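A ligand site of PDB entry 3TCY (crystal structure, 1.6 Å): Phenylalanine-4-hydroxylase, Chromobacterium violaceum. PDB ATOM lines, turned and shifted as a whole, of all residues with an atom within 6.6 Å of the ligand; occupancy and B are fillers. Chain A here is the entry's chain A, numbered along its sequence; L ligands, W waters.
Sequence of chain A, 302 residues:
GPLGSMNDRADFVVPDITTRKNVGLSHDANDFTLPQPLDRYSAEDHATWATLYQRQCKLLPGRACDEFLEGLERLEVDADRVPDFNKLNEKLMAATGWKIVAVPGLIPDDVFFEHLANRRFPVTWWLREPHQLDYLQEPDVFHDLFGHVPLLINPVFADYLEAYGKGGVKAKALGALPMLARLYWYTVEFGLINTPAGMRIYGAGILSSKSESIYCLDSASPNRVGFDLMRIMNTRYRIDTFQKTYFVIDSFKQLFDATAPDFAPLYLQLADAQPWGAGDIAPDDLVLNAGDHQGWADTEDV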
ATOM      1  N   PHE A 113     -37.886 -23.860  13.037  1.00  0.00           N
ATOM      2  CA  PHE A 113     -36.694 -23.261  12.404  1.00  0.00           C
ATOM      3  C   PHE A 113     -37.036 -22.125  11.473  1.00  0.00           C
ATOM      4  O   PHE A 113     -36.339 -21.126  11.468  1.00  0.00           O
ATOM      5  CB  PHE A 113     -35.924 -24.321  11.620  1.00  0.00           C
ATOM      6  CG  PHE A 113     -35.053 -25.175  12.467  1.00  0.00           C
ATOM      7  CD1 PHE A 113     -35.566 -26.329  13.070  1.00  0.00           C
ATOM      8  CD2 PHE A 113     -33.705 -24.885  12.628  1.00  0.00           C
ATOM      9  CE1 PHE A 113     -34.754 -27.140  13.833  1.00  0.00           C
ATOM     10  CE2 PHE A 113     -32.895 -25.709  13.392  1.00  0.00           C
ATOM     11  CZ  PHE A 113     -33.434 -26.845  14.005  1.00  0.00           C
ATOM     12  N   ASP A 159     -28.723 -12.930  16.999  1.00  0.00           N
ATOM     13  CA  ASP A 159     -28.101 -13.372  15.742  1.00  0.00           C
ATOM     14  C   ASP A 159     -27.822 -14.871  15.741  1.00  0.00           C
ATOM     15  O   ASP A 159     -28.014 -15.546  14.732  1.00  0.00           O
ATOM     16  CB  ASP A 159     -26.818 -12.597  15.453  1.00  0.00           C
ATOM     17  CG  ASP A 159     -27.063 -11.253  14.840  1.00  0.00           C
ATOM     18  OD1 ASP A 159     -28.209 -10.955  14.427  1.00  0.00           O
ATOM     19  OD2 ASP A 159     -26.098 -10.494  14.802  1.00  0.00           O
ATOM     20  N   TYR A 160     -27.384 -15.392  16.894  1.00  0.00           N
ATOM     21  CA  TYR A 160     -27.245 -16.831  17.034  1.00  0.00           C
ATOM     22  C   TYR A 160     -28.577 -17.572  16.788  1.00  0.00           C
ATOM     23  O   TYR A 160     -28.610 -18.558  16.049  1.00  0.00           O
ATOM     24  CB  TYR A 160     -26.703 -17.147  18.418  1.00  0.00           C
ATOM     25  CG  TYR A 160     -26.695 -18.612  18.784  1.00  0.00           C
ATOM     26  CD1 TYR A 160     -25.880 -19.521  18.113  1.00  0.00           C
ATOM     27  CD2 TYR A 160     -27.514 -19.095  19.808  1.00  0.00           C
ATOM     28  CE1 TYR A 160     -25.876 -20.895  18.453  1.00  0.00           C
ATOM     29  CE2 TYR A 160     -27.515 -20.459  20.157  1.00  0.00           C
ATOM     30  CZ  TYR A 160     -26.674 -21.338  19.481  1.00  0.00           C
ATOM     31  OH  TYR A 160     -26.662 -22.676  19.823  1.00  0.00           O
ATOM     32  N   LEU A 161     -29.683 -17.075  17.357  1.00  0.00           N
ATOM     33  CA  LEU A 161     -30.964 -17.758  17.125  1.00  0.00           C
ATOM     34  C   LEU A 161     -31.385 -17.701  15.655  1.00  0.00           C
ATOM     35  O   LEU A 161     -31.913 -18.673  15.126  1.00  0.00           O
ATOM     36  CB  LEU A 161     -32.082 -17.155  17.985  1.00  0.00           C
ATOM     37  CG  LEU A 161     -32.135 -17.608  19.436  1.00  0.00           C
ATOM     38  CD1 LEU A 161     -33.344 -16.933  20.040  1.00  0.00           C
ATOM     39  CD2 LEU A 161     -32.314 -19.097  19.521  1.00  0.00           C
ATOM     40  N   GLU A 162     -31.169 -16.546  15.025  1.00  0.00           N
ATOM     41  CA  GLU A 162     -31.515 -16.394  13.611  1.00  0.00           C
ATOM     42  C   GLU A 162     -30.678 -17.363  12.757  1.00  0.00           C
ATOM     43  O   GLU A 162     -31.209 -18.024  11.852  1.00  0.00           O
ATOM     44  CB  GLU A 162     -31.347 -14.930  13.163  1.00  0.00           C
ATOM     45  CG  GLU A 162     -31.705 -14.694  11.705  1.00  0.00           C
ATOM     46  CD  GLU A 162     -31.391 -13.276  11.236  1.00  0.00           C
ATOM     47  OE1 GLU A 162     -31.105 -12.418  12.088  1.00  0.00           O
ATOM     48  OE2 GLU A 162     -31.405 -13.024  10.015  1.00  0.00           O
ATOM     49  N   ALA A 163     -29.389 -17.450  13.067  1.00  0.00           N
ATOM     50  CA  ALA A 163     -28.484 -18.331  12.334  1.00  0.00           C
ATOM     51  C   ALA A 163     -28.882 -19.786  12.540  1.00  0.00           C
ATOM     52  O   ALA A 163     -28.832 -20.600  11.597  1.00  0.00           O
ATOM     53  CB  ALA A 163     -27.015 -18.094  12.760  1.00  0.00           C
ATOM     54  N   TYR A 164     -29.284 -20.102  13.771  1.00  0.00           N
ATOM     55  CA  TYR A 164     -29.738 -21.464  14.090  1.00  0.00           C
ATOM     56  C   TYR A 164     -30.958 -21.804  13.224  1.00  0.00           C
ATOM     57  O   TYR A 164     -31.006 -22.858  12.564  1.00  0.00           O
ATOM     58  CB  TYR A 164     -30.051 -21.596  15.605  1.00  0.00           C
ATOM     59  CG  TYR A 164     -30.664 -22.927  15.974  1.00  0.00           C
ATOM     60  CD1 TYR A 164     -29.853 -24.011  16.365  1.00  0.00           C
ATOM     61  CD2 TYR A 164     -32.039 -23.126  15.944  1.00  0.00           C
ATOM     62  CE1 TYR A 164     -30.392 -25.228  16.698  1.00  0.00           C
ATOM     63  CE2 TYR A 164     -32.600 -24.384  16.272  1.00  0.00           C
ATOM     64  CZ  TYR A 164     -31.761 -25.416  16.649  1.00  0.00           C
ATOM     65  OH  TYR A 164     -32.263 -26.647  16.974  1.00  0.00           O
ATOM     66  N   GLY A 165     -31.942 -20.904  13.199  1.00  0.00           N
ATOM     67  CA  GLY A 165     -33.122 -21.089  12.355  1.00  0.00           C
ATOM     68  C   GLY A 165     -32.761 -21.369  10.893  1.00  0.00           C
ATOM     69  O   GLY A 165     -33.264 -22.311  10.274  1.00  0.00           O
ATOM     70  N   LYS A 166     -31.854 -20.555  10.370  1.00  0.00           N
ATOM     71  CA  LYS A 166     -31.386 -20.692   8.986  1.00  0.00           C
ATOM     72  C   LYS A 166     -30.735 -22.031   8.743  1.00  0.00           C
ATOM     73  O   LYS A 166     -30.890 -22.604   7.667  1.00  0.00           O
ATOM     74  CB  LYS A 166     -30.448 -19.532   8.634  1.00  0.00           C
ATOM     75  CG  LYS A 166     -31.207 -18.224   8.447  1.00  0.00           C
ATOM     76  CD  LYS A 166     -30.314 -16.991   8.295  1.00  0.00           C
ATOM     77  CE  LYS A 166     -31.164 -15.759   7.951  1.00  0.00           C
ATOM     78  NZ  LYS A 166     -30.375 -14.492   7.772  1.00  0.00           N
ATOM     79  N   GLY A 167     -30.068 -22.573   9.770  1.00  0.00           N
ATOM     80  CA  GLY A 167     -29.438 -23.889   9.703  1.00  0.00           C
ATOM     81  C   GLY A 167     -30.401 -25.057   9.575  1.00  0.00           C
ATOM     82  O   GLY A 167     -30.000 -26.156   9.196  1.00  0.00           O
ATOM     83  N   GLY A 168     -31.682 -24.811   9.845  1.00  0.00           N
ATOM     84  CA  GLY A 168     -32.698 -25.871   9.772  1.00  0.00           C
ATOM     85  C   GLY A 168     -32.842 -26.562   8.436  1.00  0.00           C
ATOM     86  O   GLY A 168     -33.064 -27.771   8.388  1.00  0.00           O
ATOM     87  N   LYS A 170     -30.571 -27.057   5.998  1.00  0.00           N
ATOM     88  CA  LYS A 170     -29.480 -28.015   5.727  1.00  0.00           C
ATOM     89  C   LYS A 170     -29.663 -29.247   6.608  1.00  0.00           C
ATOM     90  O   LYS A 170     -29.478 -30.373   6.145  1.00  0.00           O
ATOM     91  CB  LYS A 170     -28.121 -27.378   6.035  1.00  0.00           C
ATOM     92  CG  LYS A 170     -26.907 -28.245   5.723  1.00  0.00           C
ATOM     93  CD  LYS A 170     -25.602 -27.569   6.176  1.00  0.00           C
ATOM     94  CE  LYS A 170     -25.313 -26.327   5.333  1.00  0.00           C
ATOM     95  NZ  LYS A 170     -24.064 -25.633   5.747  1.00  0.00           N
ATOM     96  N   ALA A 171     -30.022 -29.026   7.865  1.00  0.00           N
ATOM     97  CA  ALA A 171     -30.169 -30.143   8.803  1.00  0.00           C
ATOM     98  C   ALA A 171     -31.262 -31.088   8.358  1.00  0.00           C
ATOM     99  O   ALA A 171     -31.086 -32.310   8.372  1.00  0.00           O
ATOM    100  CB  ALA A 171     -30.461 -29.630  10.186  1.00  0.00           C
ATOM    101  N   LEU A 180     -28.979 -30.941  15.524  1.00  0.00           N
ATOM    102  CA  LEU A 180     -29.274 -29.529  15.820  1.00  0.00           C
ATOM    103  C   LEU A 180     -30.090 -29.371  17.097  1.00  0.00           C
ATOM    104  O   LEU A 180     -29.860 -28.425  17.877  1.00  0.00           O
ATOM    105  CB  LEU A 180     -29.980 -28.845  14.657  1.00  0.00           C
ATOM    106  CG  LEU A 180     -29.177 -28.064  13.634  1.00  0.00           C
ATOM    107  CD1 LEU A 180     -30.077 -27.151  12.820  1.00  0.00           C
ATOM    108  CD2 LEU A 180     -28.076 -27.263  14.275  1.00  0.00           C
ATOM    109  N   LEU A 183     -27.848 -29.306  20.056  1.00  0.00           N
ATOM    110  CA  LEU A 183     -27.191 -28.009  20.208  1.00  0.00           C
ATOM    111  C   LEU A 183     -28.124 -26.969  20.847  1.00  0.00           C
ATOM    112  O   LEU A 183     -27.718 -26.258  21.771  1.00  0.00           O
ATOM    113  CB  LEU A 183     -26.690 -27.492  18.849  1.00  0.00           C
ATOM    114  CG  LEU A 183     -26.024 -26.117  18.878  1.00  0.00           C
ATOM    115  CD1 LEU A 183     -24.757 -26.115  19.755  1.00  0.00           C
ATOM    116  CD2 LEU A 183     -25.680 -25.773  17.440  1.00  0.00           C
ATOM    117  N   LEU A 229     -18.638 -27.985  20.079  1.00  0.00           N
ATOM    118  CA  LEU A 229     -19.742 -28.196  19.112  1.00  0.00           C
ATOM    119  C   LEU A 229     -19.991 -29.674  18.757  1.00  0.00           C
ATOM    120  O   LEU A 229     -21.146 -30.139  18.777  1.00  0.00           O
ATOM    121  CB  LEU A 229     -19.518 -27.351  17.854  1.00  0.00           C
ATOM    122  CG  LEU A 229     -20.493 -27.561  16.694  1.00  0.00           C
ATOM    123  CD1 LEU A 229     -21.914 -27.142  17.100  1.00  0.00           C
ATOM    124  CD2 LEU A 229     -20.008 -26.776  15.459  1.00  0.00           C
ATOM    125  N   LEU A 255     -20.129 -18.453  21.236  1.00  0.00           N
ATOM    126  CA  LEU A 255     -21.176 -19.320  20.783  1.00  0.00           C
ATOM    127  C   LEU A 255     -21.519 -19.074  19.302  1.00  0.00           C
ATOM    128  O   LEU A 255     -21.602 -20.030  18.507  1.00  0.00           O
ATOM    129  CB  LEU A 255     -22.409 -19.161  21.690  1.00  0.00           C
ATOM    130  CG  LEU A 255     -23.639 -19.996  21.390  1.00  0.00           C
ATOM    131  CD1 LEU A 255     -23.315 -21.515  21.402  1.00  0.00           C
ATOM    132  CD2 LEU A 255     -24.711 -19.628  22.396  1.00  0.00           C
ATOM    133  N   PHE A 256     -21.615 -17.799  18.921  1.00  0.00           N
ATOM    134  CA  PHE A 256     -21.965 -17.432  17.553  1.00  0.00           C
ATOM    135  C   PHE A 256     -20.861 -17.877  16.607  1.00  0.00           C
ATOM    136  O   PHE A 256     -21.129 -18.425  15.539  1.00  0.00           O
ATOM    137  CB  PHE A 256     -22.168 -15.921  17.383  1.00  0.00           C
ATOM    138  CG  PHE A 256     -22.559 -15.536  15.985  1.00  0.00           C
ATOM    139  CD1 PHE A 256     -23.881 -15.598  15.588  1.00  0.00           C
ATOM    140  CD2 PHE A 256     -21.585 -15.176  15.048  1.00  0.00           C
ATOM    141  CE1 PHE A 256     -24.255 -15.270  14.286  1.00  0.00           C
ATOM    142  CE2 PHE A 256     -21.941 -14.851  13.738  1.00  0.00           C
ATOM    143  CZ  PHE A 256     -23.278 -14.902  13.354  1.00  0.00           C
ATOM    144  N   THR A 259     -20.327 -21.690  16.046  1.00  0.00           N
ATOM    145  CA  THR A 259     -21.393 -22.325  15.274  1.00  0.00           C
ATOM    146  C   THR A 259     -21.516 -21.775  13.856  1.00  0.00           C
ATOM    147  O   THR A 259     -22.463 -22.125  13.151  1.00  0.00           O
ATOM    148  CB  THR A 259     -22.769 -22.263  16.016  1.00  0.00           C
ATOM    149  OG1 THR A 259     -23.121 -20.893  16.301  1.00  0.00           O
ATOM    150  CG2 THR A 259     -22.730 -23.070  17.330  1.00  0.00           C
ATOM    151  N   ALA A 260     -20.553 -20.960  13.416  1.00  0.00           N
ATOM    152  CA  ALA A 260     -20.597 -20.340  12.099  1.00  0.00           C
ATOM    153  C   ALA A 260     -20.123 -21.212  10.909  1.00  0.00           C
ATOM    154  O   ALA A 260     -20.619 -21.045   9.789  1.00  0.00           O
ATOM    155  CB  ALA A 260     -19.847 -19.014  12.117  1.00  0.00           C
ATOM    156  N   PRO A 261     -19.183 -22.153  11.139  1.00  0.00           N
ATOM    157  CA  PRO A 261     -18.725 -22.972  10.015  1.00  0.00           C
ATOM    158  C   PRO A 261     -19.791 -23.942   9.460  1.00  0.00           C
ATOM    159  O   PRO A 261     -20.817 -24.163  10.097  1.00  0.00           O
ATOM    160  CB  PRO A 261     -17.575 -23.760  10.626  1.00  0.00           C
ATOM    161  CG  PRO A 261     -17.136 -22.923  11.807  1.00  0.00           C
ATOM    162  CD  PRO A 261     -18.444 -22.475  12.363  1.00  0.00           C
ATOM    163  N   ASP A 262     -19.515 -24.508   8.278  1.00  0.00           N
ATOM    164  CA  ASP A 262     -20.386 -25.478   7.609  1.00  0.00           C
ATOM    165  C   ASP A 262     -20.577 -26.734   8.457  1.00  0.00           C
ATOM    166  O   ASP A 262     -19.601 -27.452   8.746  1.00  0.00           O
ATOM    167  CB  ASP A 262     -19.762 -25.846   6.240  1.00  0.00           C
ATOM    168  CG  ASP A 262     -20.566 -26.897   5.454  1.00  0.00           C
ATOM    169  OD1 ASP A 262     -21.696 -27.208   5.856  1.00  0.00           O
ATOM    170  OD2 ASP A 262     -20.050 -27.405   4.422  1.00  0.00           O
ATOM    171  N   PHE A 263     -21.823 -27.016   8.830  1.00  0.00           N
ATOM    172  CA  PHE A 263     -22.096 -28.187   9.677  1.00  0.00           C
ATOM    173  C   PHE A 263     -22.205 -29.492   8.886  1.00  0.00           C
ATOM    174  O   PHE A 263     -22.249 -30.568   9.494  1.00  0.00           O
ATOM    175  CB  PHE A 263     -23.400 -28.017  10.460  1.00  0.00           C
ATOM    176  CG  PHE A 263     -23.296 -27.137  11.689  1.00  0.00           C
ATOM    177  CD1 PHE A 263     -24.306 -27.201  12.658  1.00  0.00           C
ATOM    178  CD2 PHE A 263     -22.211 -26.269  11.887  1.00  0.00           C
ATOM    179  CE1 PHE A 263     -24.265 -26.373  13.786  1.00  0.00           C
ATOM    180  CE2 PHE A 263     -22.162 -25.464  13.020  1.00  0.00           C
ATOM    181  CZ  PHE A 263     -23.182 -25.508  13.954  1.00  0.00           C
ATOM    182  N   ALA A 264     -22.267 -29.417   7.556  1.00  0.00           N
ATOM    183  CA  ALA A 264     -22.525 -30.621   6.753  1.00  0.00           C
ATOM    184  C   ALA A 264     -21.525 -31.776   7.022  1.00  0.00           C
ATOM    185  O   ALA A 264     -21.957 -32.901   7.304  1.00  0.00           O
ATOM    186  CB  ALA A 264     -22.616 -30.298   5.285  1.00  0.00           C
ATOM    187  N   TYR A 267     -22.200 -33.199  10.558  1.00  0.00           N
ATOM    188  CA  TYR A 267     -23.344 -34.108  10.556  1.00  0.00           C
ATOM    189  C   TYR A 267     -22.994 -35.486  10.004  1.00  0.00           C
ATOM    190  O   TYR A 267     -23.386 -36.512  10.572  1.00  0.00           O
ATOM    191  CB  TYR A 267     -24.474 -33.538   9.701  1.00  0.00           C
ATOM    192  CG  TYR A 267     -25.132 -32.276  10.205  1.00  0.00           C
ATOM    193  CD1 TYR A 267     -25.640 -31.343   9.292  1.00  0.00           C
ATOM    194  CD2 TYR A 267     -25.266 -32.001  11.555  1.00  0.00           C
ATOM    195  CE1 TYR A 267     -26.279 -30.187   9.708  1.00  0.00           C
ATOM    196  CE2 TYR A 267     -25.907 -30.850  11.995  1.00  0.00           C
ATOM    197  CZ  TYR A 267     -26.393 -29.943  11.067  1.00  0.00           C
ATOM    198  OH  TYR A 267     -27.023 -28.800  11.511  1.00  0.00           O
HETATM  199  N1  LIG L   1     -23.362 -23.167  10.668  1.00  0.00           N
HETATM  200  C1  LIG L   1     -24.563 -24.008  10.548  1.00  0.00           C
HETATM  201  C2  LIG L   1     -24.685 -24.627   9.176  1.00  0.00           C
HETATM  202  O1  LIG L   1     -23.708 -24.719   8.443  1.00  0.00           O
HETATM  203  C3  LIG L   1     -25.841 -23.195  10.813  1.00  0.00           C
HETATM  204  C4  LIG L   1     -26.054 -22.958  12.284  1.00  0.00           C
HETATM  205  C5  LIG L   1     -26.553 -23.983  13.097  1.00  0.00           C
HETATM  206  C6  LIG L   1     -25.779 -21.696  12.807  1.00  0.00           C
HETATM  207  C7  LIG L   1     -26.740 -23.734  14.464  1.00  0.00           C
HETATM  208  C8  LIG L   1     -25.970 -21.454  14.168  1.00  0.00           C
HETATM  209  C9  LIG L   1     -26.445 -22.482  14.987  1.00  0.00           C
HETATM  210  O2  LIG L   1     -25.809 -25.053   8.827  1.00  0.00           O
HETATM  211  O   HOH W   1     -26.959 -23.897   6.838  1.00  0.00           O
HETATM  212  O   HOH W   2     -27.424 -26.940   9.524  1.00  0.00           O
HETATM  213  O   HOH W   3     -22.266 -22.161   6.573  1.00  0.00           O
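The backbone carbonyl oxygen (O) of Leu 255 sits at hydrogen-bond distance from the side-chain hydroxyl (OG1) of Thr 259 (2.8 Å).
OH of Tyr 164 lies within hydrogen-bond range of O of Leu 180, 3.1 Å away.
The side-chain carboxylate of Asp 262 is in salt-bridge range of the side-chain amino group of Lys 170 (2.8 Å).
The side-chain carboxylate (OD1) of Asp 262 lies within hydrogen-bond range of the backbone NH (N) of Ala 264, 2.8 Å away.
The side-chain hydroxyl (OG1) of Thr 259 sits at hydrogen-bond distance from the backbone carbonyl oxygen (O) of Phe 256.
O1 of the ligand sits at hydrogen-bond distance from N of Phe 263 (3.0 Å).
N1 of the ligand sits at hydrogen-bond distance from O of Thr 259, at 2.8 Å.
N1 of the ligand is in hydrogen-bond range of O of Pro 261, at 2.8 Å.
An oxygen (O1) of the ligand lies within salt-bridge range of the side-chain amino group (NZ) of Lys 170 (2.9 Å).
Water W2 lies within hydrogen-bond range of O2 of the ligand, O of Gly 167 and OH of Tyr 267.
Tyr 160 touches the ligand (CE1 to C9, 3.9 Å).
Ala 163 touches the ligand.
CA of Tyr 164 touches C9 of the ligand, 3.6 Å away.
CA of Gly 167 touches C3 of the ligand, at 3.8 Å.
CD2 of Leu 180 touches C7 of the ligand, 3.8 Å away.
Leu 183 touches the ligand.
Ala 260 touches the ligand.
Asp 262 touches the ligand.
Of the 25 residues printed, 12 come within 4 Å of the ligand.
Along chain A the residues within 4 Å of the ligand span positions 160 to 263.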
